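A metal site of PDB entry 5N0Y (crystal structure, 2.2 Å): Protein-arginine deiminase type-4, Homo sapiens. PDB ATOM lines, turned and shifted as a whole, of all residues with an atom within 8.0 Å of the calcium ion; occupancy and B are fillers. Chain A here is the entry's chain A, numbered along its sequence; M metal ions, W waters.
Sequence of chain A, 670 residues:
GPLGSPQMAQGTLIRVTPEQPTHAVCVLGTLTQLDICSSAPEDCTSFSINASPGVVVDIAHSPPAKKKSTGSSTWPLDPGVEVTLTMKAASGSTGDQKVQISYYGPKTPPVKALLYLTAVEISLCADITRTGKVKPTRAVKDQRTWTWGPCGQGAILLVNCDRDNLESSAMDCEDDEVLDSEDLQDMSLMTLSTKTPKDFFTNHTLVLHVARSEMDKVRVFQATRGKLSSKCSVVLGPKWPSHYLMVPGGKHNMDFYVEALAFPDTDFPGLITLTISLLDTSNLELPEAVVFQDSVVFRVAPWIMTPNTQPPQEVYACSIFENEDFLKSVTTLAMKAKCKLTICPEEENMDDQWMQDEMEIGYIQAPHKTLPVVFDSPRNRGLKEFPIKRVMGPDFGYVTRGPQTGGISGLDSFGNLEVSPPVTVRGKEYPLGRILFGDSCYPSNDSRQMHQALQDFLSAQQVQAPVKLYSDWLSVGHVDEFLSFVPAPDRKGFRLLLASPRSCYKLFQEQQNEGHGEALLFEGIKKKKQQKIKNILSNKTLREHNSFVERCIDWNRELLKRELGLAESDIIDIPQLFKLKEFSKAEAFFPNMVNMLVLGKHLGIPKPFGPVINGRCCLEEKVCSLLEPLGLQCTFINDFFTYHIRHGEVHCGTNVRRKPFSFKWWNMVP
The backbone carbonyl oxygen of Asp 376 sits at hydrogen-bond distance from the side-chain hydroxyl of Thr 400 (2.8 Å).
The side-chain hydroxyl of Tyr 398 sits at hydrogen-bond distance from the side-chain carboxylate of Asp 376, at 2.7 Å.
N of Asp 376 lies within hydrogen-bond range of O of Val 399 (3.0 Å).
N of Arg 379 lies close to OG of Ser 377, 3.1 Å away.
The side-chain amide nitrogen (ND2) of Asn 380 lies close to the backbone carbonyl oxygen (O) of Pro 378, at 3.5 Å.
The side-chain amide nitrogen (ND2) of Asn 380 sits at hydrogen-bond distance from the backbone carbonyl oxygen (O) of Gln 404, at 2.8 Å.
NH2 of Arg 379 lies within salt-bridge range of OE2 of Glu 358.
The side-chain carboxylate (OE2) of Glu 358 lies within hydrogen-bond range of the backbone NH (N) of Arg 381 (3.4 Å).
Four residues have an atom within 4 Å of the calcium ion: Glu 358, Asp 376, Ser 377 and Asn 380.
The calcium ion is bound by OD1 of Asp 376 (2.2 Å), O of Ser 377 (2.3 Å), water W1 (2.4 Å), OD1 of Asn 380 (2.4 Å), OE1 of Glu 358 (2.5 Å) and water W2 (2.5 Å).
Water W2 lies within hydrogen-bond range of OE1 of Gln 404 (2.8 Å), OG1 of Thr 400 (3.0 Å) and OD2 of Asp 376 (3.3 Å).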
ATOM      1  N   ASP A 357     -21.171  24.409 -12.791  1.00  0.00           N
ATOM      2  CA  ASP A 357     -21.695  24.619 -14.121  1.00  0.00           C
ATOM      3  C   ASP A 357     -22.853  25.619 -14.244  1.00  0.00           C
ATOM      4  O   ASP A 357     -23.049  26.213 -15.339  1.00  0.00           O
ATOM      5  CB  ASP A 357     -22.042  23.268 -14.744  1.00  0.00           C
ATOM      6  CG  ASP A 357     -20.783  22.474 -15.156  1.00  0.00           C
ATOM      7  OD1 ASP A 357     -19.689  23.119 -15.310  1.00  0.00           O
ATOM      8  OD2 ASP A 357     -20.886  21.226 -15.311  1.00  0.00           O
ATOM      9  N   GLU A 358     -23.594  25.825 -13.157  1.00  0.00           N
ATOM     10  CA  GLU A 358     -24.812  26.600 -13.253  1.00  0.00           C
ATOM     11  C   GLU A 358     -24.512  28.061 -12.960  1.00  0.00           C
ATOM     12  O   GLU A 358     -25.316  28.922 -13.304  1.00  0.00           O
ATOM     13  CB  GLU A 358     -25.892  26.080 -12.274  1.00  0.00           C
ATOM     14  CG  GLU A 358     -27.322  26.623 -12.482  1.00  0.00           C
ATOM     15  CD  GLU A 358     -28.048  26.064 -13.715  1.00  0.00           C
ATOM     16  OE1 GLU A 358     -28.978  26.772 -14.191  1.00  0.00           O
ATOM     17  OE2 GLU A 358     -27.695  24.971 -14.224  1.00  0.00           O
ATOM     18  N   MET A 359     -23.365  28.371 -12.356  1.00  0.00           N
ATOM     19  CA  MET A 359     -23.112  29.753 -11.970  1.00  0.00           C
ATOM     20  C   MET A 359     -21.652  30.190 -11.963  1.00  0.00           C
ATOM     21  O   MET A 359     -20.754  29.350 -11.935  1.00  0.00           O
ATOM     22  CB  MET A 359     -23.722  29.983 -10.595  1.00  0.00           C
ATOM     23  CG  MET A 359     -22.911  29.533  -9.422  1.00  0.00           C
ATOM     24  SD  MET A 359     -23.869  29.623  -7.872  1.00  0.00           S
ATOM     25  CE  MET A 359     -22.548  29.338  -6.688  1.00  0.00           C
ATOM     26  N   PHE A 375     -23.404  35.276 -11.889  1.00  0.00           N
ATOM     27  CA  PHE A 375     -23.828  35.190 -13.227  1.00  0.00           C
ATOM     28  C   PHE A 375     -24.347  33.777 -13.316  1.00  0.00           C
ATOM     29  O   PHE A 375     -23.615  32.852 -13.076  1.00  0.00           O
ATOM     30  CB  PHE A 375     -22.676  35.485 -14.161  1.00  0.00           C
ATOM     31  CG  PHE A 375     -23.022  35.466 -15.611  1.00  0.00           C
ATOM     32  CD1 PHE A 375     -24.322  35.622 -16.049  1.00  0.00           C
ATOM     33  CD2 PHE A 375     -22.011  35.326 -16.582  1.00  0.00           C
ATOM     34  CE1 PHE A 375     -24.609  35.625 -17.399  1.00  0.00           C
ATOM     35  CE2 PHE A 375     -22.313  35.337 -17.938  1.00  0.00           C
ATOM     36  CZ  PHE A 375     -23.610  35.482 -18.349  1.00  0.00           C
ATOM     37  N   ASP A 376     -25.641  33.645 -13.619  1.00  0.00           N
ATOM     38  CA  ASP A 376     -26.388  32.407 -13.605  1.00  0.00           C
ATOM     39  C   ASP A 376     -26.508  31.944 -15.047  1.00  0.00           C
ATOM     40  O   ASP A 376     -26.959  32.656 -15.919  1.00  0.00           O
ATOM     41  CB  ASP A 376     -27.764  32.723 -13.023  1.00  0.00           C
ATOM     42  CG  ASP A 376     -28.709  31.508 -12.914  1.00  0.00           C
ATOM     43  OD1 ASP A 376     -28.446  30.389 -13.391  1.00  0.00           O
ATOM     44  OD2 ASP A 376     -29.791  31.725 -12.336  1.00  0.00           O
ATOM     45  N   SER A 377     -26.110  30.714 -15.280  1.00  0.00           N
ATOM     46  CA  SER A 377     -25.989  30.218 -16.610  1.00  0.00           C
ATOM     47  C   SER A 377     -27.354  29.783 -17.079  1.00  0.00           C
ATOM     48  O   SER A 377     -28.130  29.203 -16.317  1.00  0.00           O
ATOM     49  CB  SER A 377     -25.012  29.015 -16.602  1.00  0.00           C
ATOM     50  OG  SER A 377     -25.087  28.234 -17.796  1.00  0.00           O
ATOM     51  N   PRO A 378     -27.639  29.949 -18.354  1.00  0.00           N
ATOM     52  CA  PRO A 378     -28.896  29.409 -18.843  1.00  0.00           C
ATOM     53  C   PRO A 378     -28.947  27.879 -18.909  1.00  0.00           C
ATOM     54  O   PRO A 378     -29.900  27.335 -19.410  1.00  0.00           O
ATOM     55  CB  PRO A 378     -28.996  29.999 -20.253  1.00  0.00           C
ATOM     56  CG  PRO A 378     -27.572  30.108 -20.695  1.00  0.00           C
ATOM     57  CD  PRO A 378     -26.790  30.461 -19.452  1.00  0.00           C
ATOM     58  N   ARG A 379     -27.888  27.188 -18.482  1.00  0.00           N
ATOM     59  CA  ARG A 379     -27.899  25.737 -18.294  1.00  0.00           C
ATOM     60  C   ARG A 379     -29.257  25.208 -17.786  1.00  0.00           C
ATOM     61  O   ARG A 379     -29.875  24.368 -18.428  1.00  0.00           O
ATOM     62  CB  ARG A 379     -26.763  25.343 -17.328  1.00  0.00           C
ATOM     63  CG  ARG A 379     -26.491  23.858 -17.248  1.00  0.00           C
ATOM     64  CD  ARG A 379     -25.302  23.643 -16.346  1.00  0.00           C
ATOM     65  NE  ARG A 379     -25.174  22.266 -15.863  1.00  0.00           N
ATOM     66  CZ  ARG A 379     -25.541  21.822 -14.650  1.00  0.00           C
ATOM     67  NH1 ARG A 379     -25.341  20.554 -14.326  1.00  0.00           N
ATOM     68  NH2 ARG A 379     -26.093  22.633 -13.744  1.00  0.00           N
ATOM     69  N   ASN A 380     -29.714  25.742 -16.665  1.00  0.00           N
ATOM     70  CA  ASN A 380     -31.065  25.419 -16.120  1.00  0.00           C
ATOM     71  C   ASN A 380     -31.344  23.899 -15.931  1.00  0.00           C
ATOM     72  O   ASN A 380     -32.330  23.371 -16.401  1.00  0.00           O
ATOM     73  CB  ASN A 380     -32.153  26.084 -16.985  1.00  0.00           C
ATOM     74  CG  ASN A 380     -32.139  27.614 -16.884  1.00  0.00           C
ATOM     75  OD1 ASN A 380     -31.511  28.181 -15.972  1.00  0.00           O
ATOM     76  ND2 ASN A 380     -32.860  28.295 -17.814  1.00  0.00           N
ATOM     77  N   ARG A 381     -30.445  23.219 -15.256  1.00  0.00           N
ATOM     78  CA  ARG A 381     -30.709  21.854 -14.825  1.00  0.00           C
ATOM     79  C   ARG A 381     -31.179  21.897 -13.355  1.00  0.00           C
ATOM     80  O   ARG A 381     -31.684  22.918 -12.891  1.00  0.00           O
ATOM     81  CB  ARG A 381     -29.454  20.995 -15.068  1.00  0.00           C
ATOM     82  CG  ARG A 381     -29.325  20.620 -16.523  1.00  0.00           C
ATOM     83  CD  ARG A 381     -28.153  19.701 -16.759  1.00  0.00           C
ATOM     84  NE  ARG A 381     -28.313  19.096 -18.091  1.00  0.00           N
ATOM     85  CZ  ARG A 381     -27.691  17.989 -18.526  1.00  0.00           C
ATOM     86  NH1 ARG A 381     -27.943  17.532 -19.758  1.00  0.00           N
ATOM     87  NH2 ARG A 381     -26.785  17.371 -17.763  1.00  0.00           N
ATOM     88  N   LEU A 383     -29.858  22.538 -10.545  1.00  0.00           N
ATOM     89  CA  LEU A 383     -29.422  23.641  -9.673  1.00  0.00           C
ATOM     90  C   LEU A 383     -30.053  24.979 -10.064  1.00  0.00           C
ATOM     91  O   LEU A 383     -29.787  25.986  -9.395  1.00  0.00           O
ATOM     92  CB  LEU A 383     -27.903  23.771  -9.643  1.00  0.00           C
ATOM     93  CG  LEU A 383     -27.180  22.812  -8.714  1.00  0.00           C
ATOM     94  CD1 LEU A 383     -25.763  22.561  -9.231  1.00  0.00           C
ATOM     95  CD2 LEU A 383     -27.180  23.340  -7.287  1.00  0.00           C
ATOM     96  N   LYS A 384     -30.903  24.960 -11.104  1.00  0.00           N
ATOM     97  CA  LYS A 384     -31.644  26.117 -11.652  1.00  0.00           C
ATOM     98  C   LYS A 384     -32.038  27.203 -10.634  1.00  0.00           C
ATOM     99  O   LYS A 384     -31.890  28.389 -10.908  1.00  0.00           O
ATOM    100  CB  LYS A 384     -32.896  25.613 -12.407  1.00  0.00           C
ATOM    101  CG  LYS A 384     -33.928  26.669 -12.748  1.00  0.00           C
ATOM    102  CD  LYS A 384     -34.963  26.176 -13.760  1.00  0.00           C
ATOM    103  CE  LYS A 384     -36.090  27.209 -13.916  1.00  0.00           C
ATOM    104  NZ  LYS A 384     -36.487  27.402 -15.331  1.00  0.00           N
ATOM    105  N   GLU A 385     -32.508  26.795  -9.460  1.00  0.00           N
ATOM    106  CA  GLU A 385     -33.021  27.715  -8.451  1.00  0.00           C
ATOM    107  C   GLU A 385     -31.967  28.277  -7.544  1.00  0.00           C
ATOM    108  O   GLU A 385     -32.145  29.396  -7.022  1.00  0.00           O
ATOM    109  CB  GLU A 385     -34.105  27.020  -7.605  1.00  0.00           C
ATOM    110  CG  GLU A 385     -35.363  26.723  -8.420  1.00  0.00           C
ATOM    111  CD  GLU A 385     -35.897  27.963  -9.129  1.00  0.00           C
ATOM    112  OE1 GLU A 385     -36.218  27.874 -10.339  1.00  0.00           O
ATOM    113  OE2 GLU A 385     -35.962  29.034  -8.476  1.00  0.00           O
ATOM    114  N   PHE A 386     -30.891  27.529  -7.379  1.00  0.00           N
ATOM    115  CA  PHE A 386     -29.866  27.837  -6.373  1.00  0.00           C
ATOM    116  C   PHE A 386     -29.353  29.288  -6.431  1.00  0.00           C
ATOM    117  O   PHE A 386     -29.221  29.929  -5.373  1.00  0.00           O
ATOM    118  CB  PHE A 386     -28.681  26.816  -6.445  1.00  0.00           C
ATOM    119  CG  PHE A 386     -27.660  27.026  -5.360  1.00  0.00           C
ATOM    120  CD1 PHE A 386     -27.992  26.763  -4.024  1.00  0.00           C
ATOM    121  CD2 PHE A 386     -26.374  27.509  -5.662  1.00  0.00           C
ATOM    122  CE1 PHE A 386     -27.055  26.975  -3.015  1.00  0.00           C
ATOM    123  CE2 PHE A 386     -25.437  27.721  -4.653  1.00  0.00           C
ATOM    124  CZ  PHE A 386     -25.783  27.442  -3.322  1.00  0.00           C
ATOM    125  N   PRO A 387     -29.053  29.803  -7.663  1.00  0.00           N
ATOM    126  CA  PRO A 387     -28.575  31.171  -7.739  1.00  0.00           C
ATOM    127  C   PRO A 387     -29.639  32.206  -7.339  1.00  0.00           C
ATOM    128  O   PRO A 387     -29.321  33.165  -6.609  1.00  0.00           O
ATOM    129  CB  PRO A 387     -28.186  31.318  -9.212  1.00  0.00           C
ATOM    130  CG  PRO A 387     -27.932  29.917  -9.669  1.00  0.00           C
ATOM    131  CD  PRO A 387     -29.040  29.186  -8.986  1.00  0.00           C
ATOM    132  N   ILE A 388     -30.868  31.967  -7.789  1.00  0.00           N
ATOM    133  CA  ILE A 388     -31.993  32.849  -7.497  1.00  0.00           C
ATOM    134  C   ILE A 388     -32.337  32.811  -5.997  1.00  0.00           C
ATOM    135  O   ILE A 388     -32.419  33.869  -5.336  1.00  0.00           O
ATOM    136  CB  ILE A 388     -33.260  32.450  -8.286  1.00  0.00           C
ATOM    137  CG1 ILE A 388     -32.987  32.499  -9.785  1.00  0.00           C
ATOM    138  CG2 ILE A 388     -34.429  33.366  -7.933  1.00  0.00           C
ATOM    139  CD1 ILE A 388     -33.950  31.665 -10.604  1.00  0.00           C
ATOM    140  N   TYR A 398     -27.334  39.589  -8.822  1.00  0.00           N
ATOM    141  CA  TYR A 398     -27.734  38.561  -9.766  1.00  0.00           C
ATOM    142  C   TYR A 398     -27.784  39.081 -11.230  1.00  0.00           C
ATOM    143  O   TYR A 398     -28.171  40.212 -11.469  1.00  0.00           O
ATOM    144  CB  TYR A 398     -29.106  38.028  -9.344  1.00  0.00           C
ATOM    145  CG  TYR A 398     -29.632  36.981 -10.260  1.00  0.00           C
ATOM    146  CD1 TYR A 398     -29.382  35.650 -10.032  1.00  0.00           C
ATOM    147  CD2 TYR A 398     -30.413  37.334 -11.367  1.00  0.00           C
ATOM    148  CE1 TYR A 398     -29.868  34.689 -10.875  1.00  0.00           C
ATOM    149  CE2 TYR A 398     -30.881  36.361 -12.217  1.00  0.00           C
ATOM    150  CZ  TYR A 398     -30.588  35.052 -11.962  1.00  0.00           C
ATOM    151  OH  TYR A 398     -31.050  34.089 -12.798  1.00  0.00           O
ATOM    152  N   VAL A 399     -27.385  38.226 -12.190  1.00  0.00           N
ATOM    153  CA  VAL A 399     -27.485  38.521 -13.618  1.00  0.00           C
ATOM    154  C   VAL A 399     -27.658  37.247 -14.369  1.00  0.00           C
ATOM    155  O   VAL A 399     -27.041  36.245 -14.039  1.00  0.00           O
ATOM    156  CB  VAL A 399     -26.177  39.025 -14.293  1.00  0.00           C
ATOM    157  CG1 VAL A 399     -26.511  39.998 -15.419  1.00  0.00           C
ATOM    158  CG2 VAL A 399     -25.169  39.604 -13.341  1.00  0.00           C
ATOM    159  N   THR A 400     -28.402  37.294 -15.459  1.00  0.00           N
ATOM    160  CA  THR A 400     -28.485  36.128 -16.318  1.00  0.00           C
ATOM    161  C   THR A 400     -28.584  36.522 -17.804  1.00  0.00           C
ATOM    162  O   THR A 400     -29.058  37.573 -18.130  1.00  0.00           O
ATOM    163  CB  THR A 400     -29.647  35.204 -15.866  1.00  0.00           C
ATOM    164  OG1 THR A 400     -29.377  33.893 -16.366  1.00  0.00           O
ATOM    165  CG2 THR A 400     -31.033  35.665 -16.381  1.00  0.00           C
ATOM    166  N   ARG A 401     -28.144  35.636 -18.673  1.00  0.00           N
ATOM    167  CA  ARG A 401     -28.222  35.889 -20.119  1.00  0.00           C
ATOM    168  C   ARG A 401     -28.583  34.641 -20.905  1.00  0.00           C
ATOM    169  O   ARG A 401     -28.473  33.527 -20.404  1.00  0.00           O
ATOM    170  CB  ARG A 401     -26.875  36.419 -20.615  1.00  0.00           C
ATOM    171  CG  ARG A 401     -26.625  37.881 -20.274  1.00  0.00           C
ATOM    172  CD  ARG A 401     -27.697  38.722 -20.888  1.00  0.00           C
ATOM    173  NE  ARG A 401     -27.486  40.131 -20.693  1.00  0.00           N
ATOM    174  CZ  ARG A 401     -27.751  40.800 -19.593  1.00  0.00           C
ATOM    175  NH1 ARG A 401     -28.194  40.192 -18.511  1.00  0.00           N
ATOM    176  NH2 ARG A 401     -27.536  42.095 -19.572  1.00  0.00           N
ATOM    177  N   PRO A 403     -31.155  32.237 -23.691  1.00  0.00           N
ATOM    178  CA  PRO A 403     -32.530  31.769 -23.610  1.00  0.00           C
ATOM    179  C   PRO A 403     -32.652  30.789 -22.460  1.00  0.00           C
ATOM    180  O   PRO A 403     -31.775  29.942 -22.280  1.00  0.00           O
ATOM    181  CB  PRO A 403     -32.749  31.056 -24.935  1.00  0.00           C
ATOM    182  CG  PRO A 403     -31.397  30.654 -25.408  1.00  0.00           C
ATOM    183  CD  PRO A 403     -30.431  31.664 -24.845  1.00  0.00           C
ATOM    184  N   GLN A 404     -33.733  30.928 -21.708  1.00  0.00           N
ATOM    185  CA  GLN A 404     -33.957  30.165 -20.484  1.00  0.00           C
ATOM    186  C   GLN A 404     -34.694  28.834 -20.712  1.00  0.00           C
ATOM    187  O   GLN A 404     -34.749  28.012 -19.809  1.00  0.00           O
ATOM    188  CB  GLN A 404     -34.650  31.061 -19.444  1.00  0.00           C
ATOM    189  CG  GLN A 404     -33.824  32.275 -19.066  1.00  0.00           C
ATOM    190  CD  GLN A 404     -32.462  31.936 -18.447  1.00  0.00           C
ATOM    191  OE1 GLN A 404     -32.358  31.068 -17.579  1.00  0.00           O
ATOM    192  NE2 GLN A 404     -31.420  32.623 -18.892  1.00  0.00           N
ATOM    193  N   ILE A 408     -29.607  26.064 -26.274  1.00  0.00           N
ATOM    194  CA  ILE A 408     -28.444  26.088 -25.395  1.00  0.00           C
ATOM    195  C   ILE A 408     -27.493  24.946 -25.825  1.00  0.00           C
ATOM    196  O   ILE A 408     -27.809  24.176 -26.730  1.00  0.00           O
ATOM    197  CB  ILE A 408     -28.983  25.887 -23.949  1.00  0.00           C
ATOM    198  CG1 ILE A 408     -27.874  25.928 -22.928  1.00  0.00           C
ATOM    199  CG2 ILE A 408     -29.772  24.569 -23.778  1.00  0.00           C
ATOM    200  CD1 ILE A 408     -28.416  25.994 -21.539  1.00  0.00           C
ATOM    201  N   PHE A 414     -20.758  26.805 -16.925  1.00  0.00           N
ATOM    202  CA  PHE A 414     -19.692  27.724 -16.505  1.00  0.00           C
ATOM    203  C   PHE A 414     -18.383  27.112 -16.041  1.00  0.00           C
ATOM    204  O   PHE A 414     -17.463  27.831 -15.641  1.00  0.00           O
ATOM    205  CB  PHE A 414     -20.211  28.784 -15.570  1.00  0.00           C
ATOM    206  CG  PHE A 414     -21.173  29.773 -16.225  1.00  0.00           C
ATOM    207  CD1 PHE A 414     -21.468  29.750 -17.606  1.00  0.00           C
ATOM    208  CD2 PHE A 414     -21.733  30.783 -15.446  1.00  0.00           C
ATOM    209  CE1 PHE A 414     -22.303  30.690 -18.163  1.00  0.00           C
ATOM    210  CE2 PHE A 414     -22.578  31.744 -16.006  1.00  0.00           C
ATOM    211  CZ  PHE A 414     -22.869  31.685 -17.358  1.00  0.00           C
HETATM  212 CA    CA M   1     -29.694  29.077 -14.669  1.00  0.00          CA
HETATM  213  O   HOH W   1     -31.415  29.283 -13.079  1.00  0.00           O
HETATM  214  O   HOH W   2     -30.489  31.247 -15.537  1.00  0.00           O
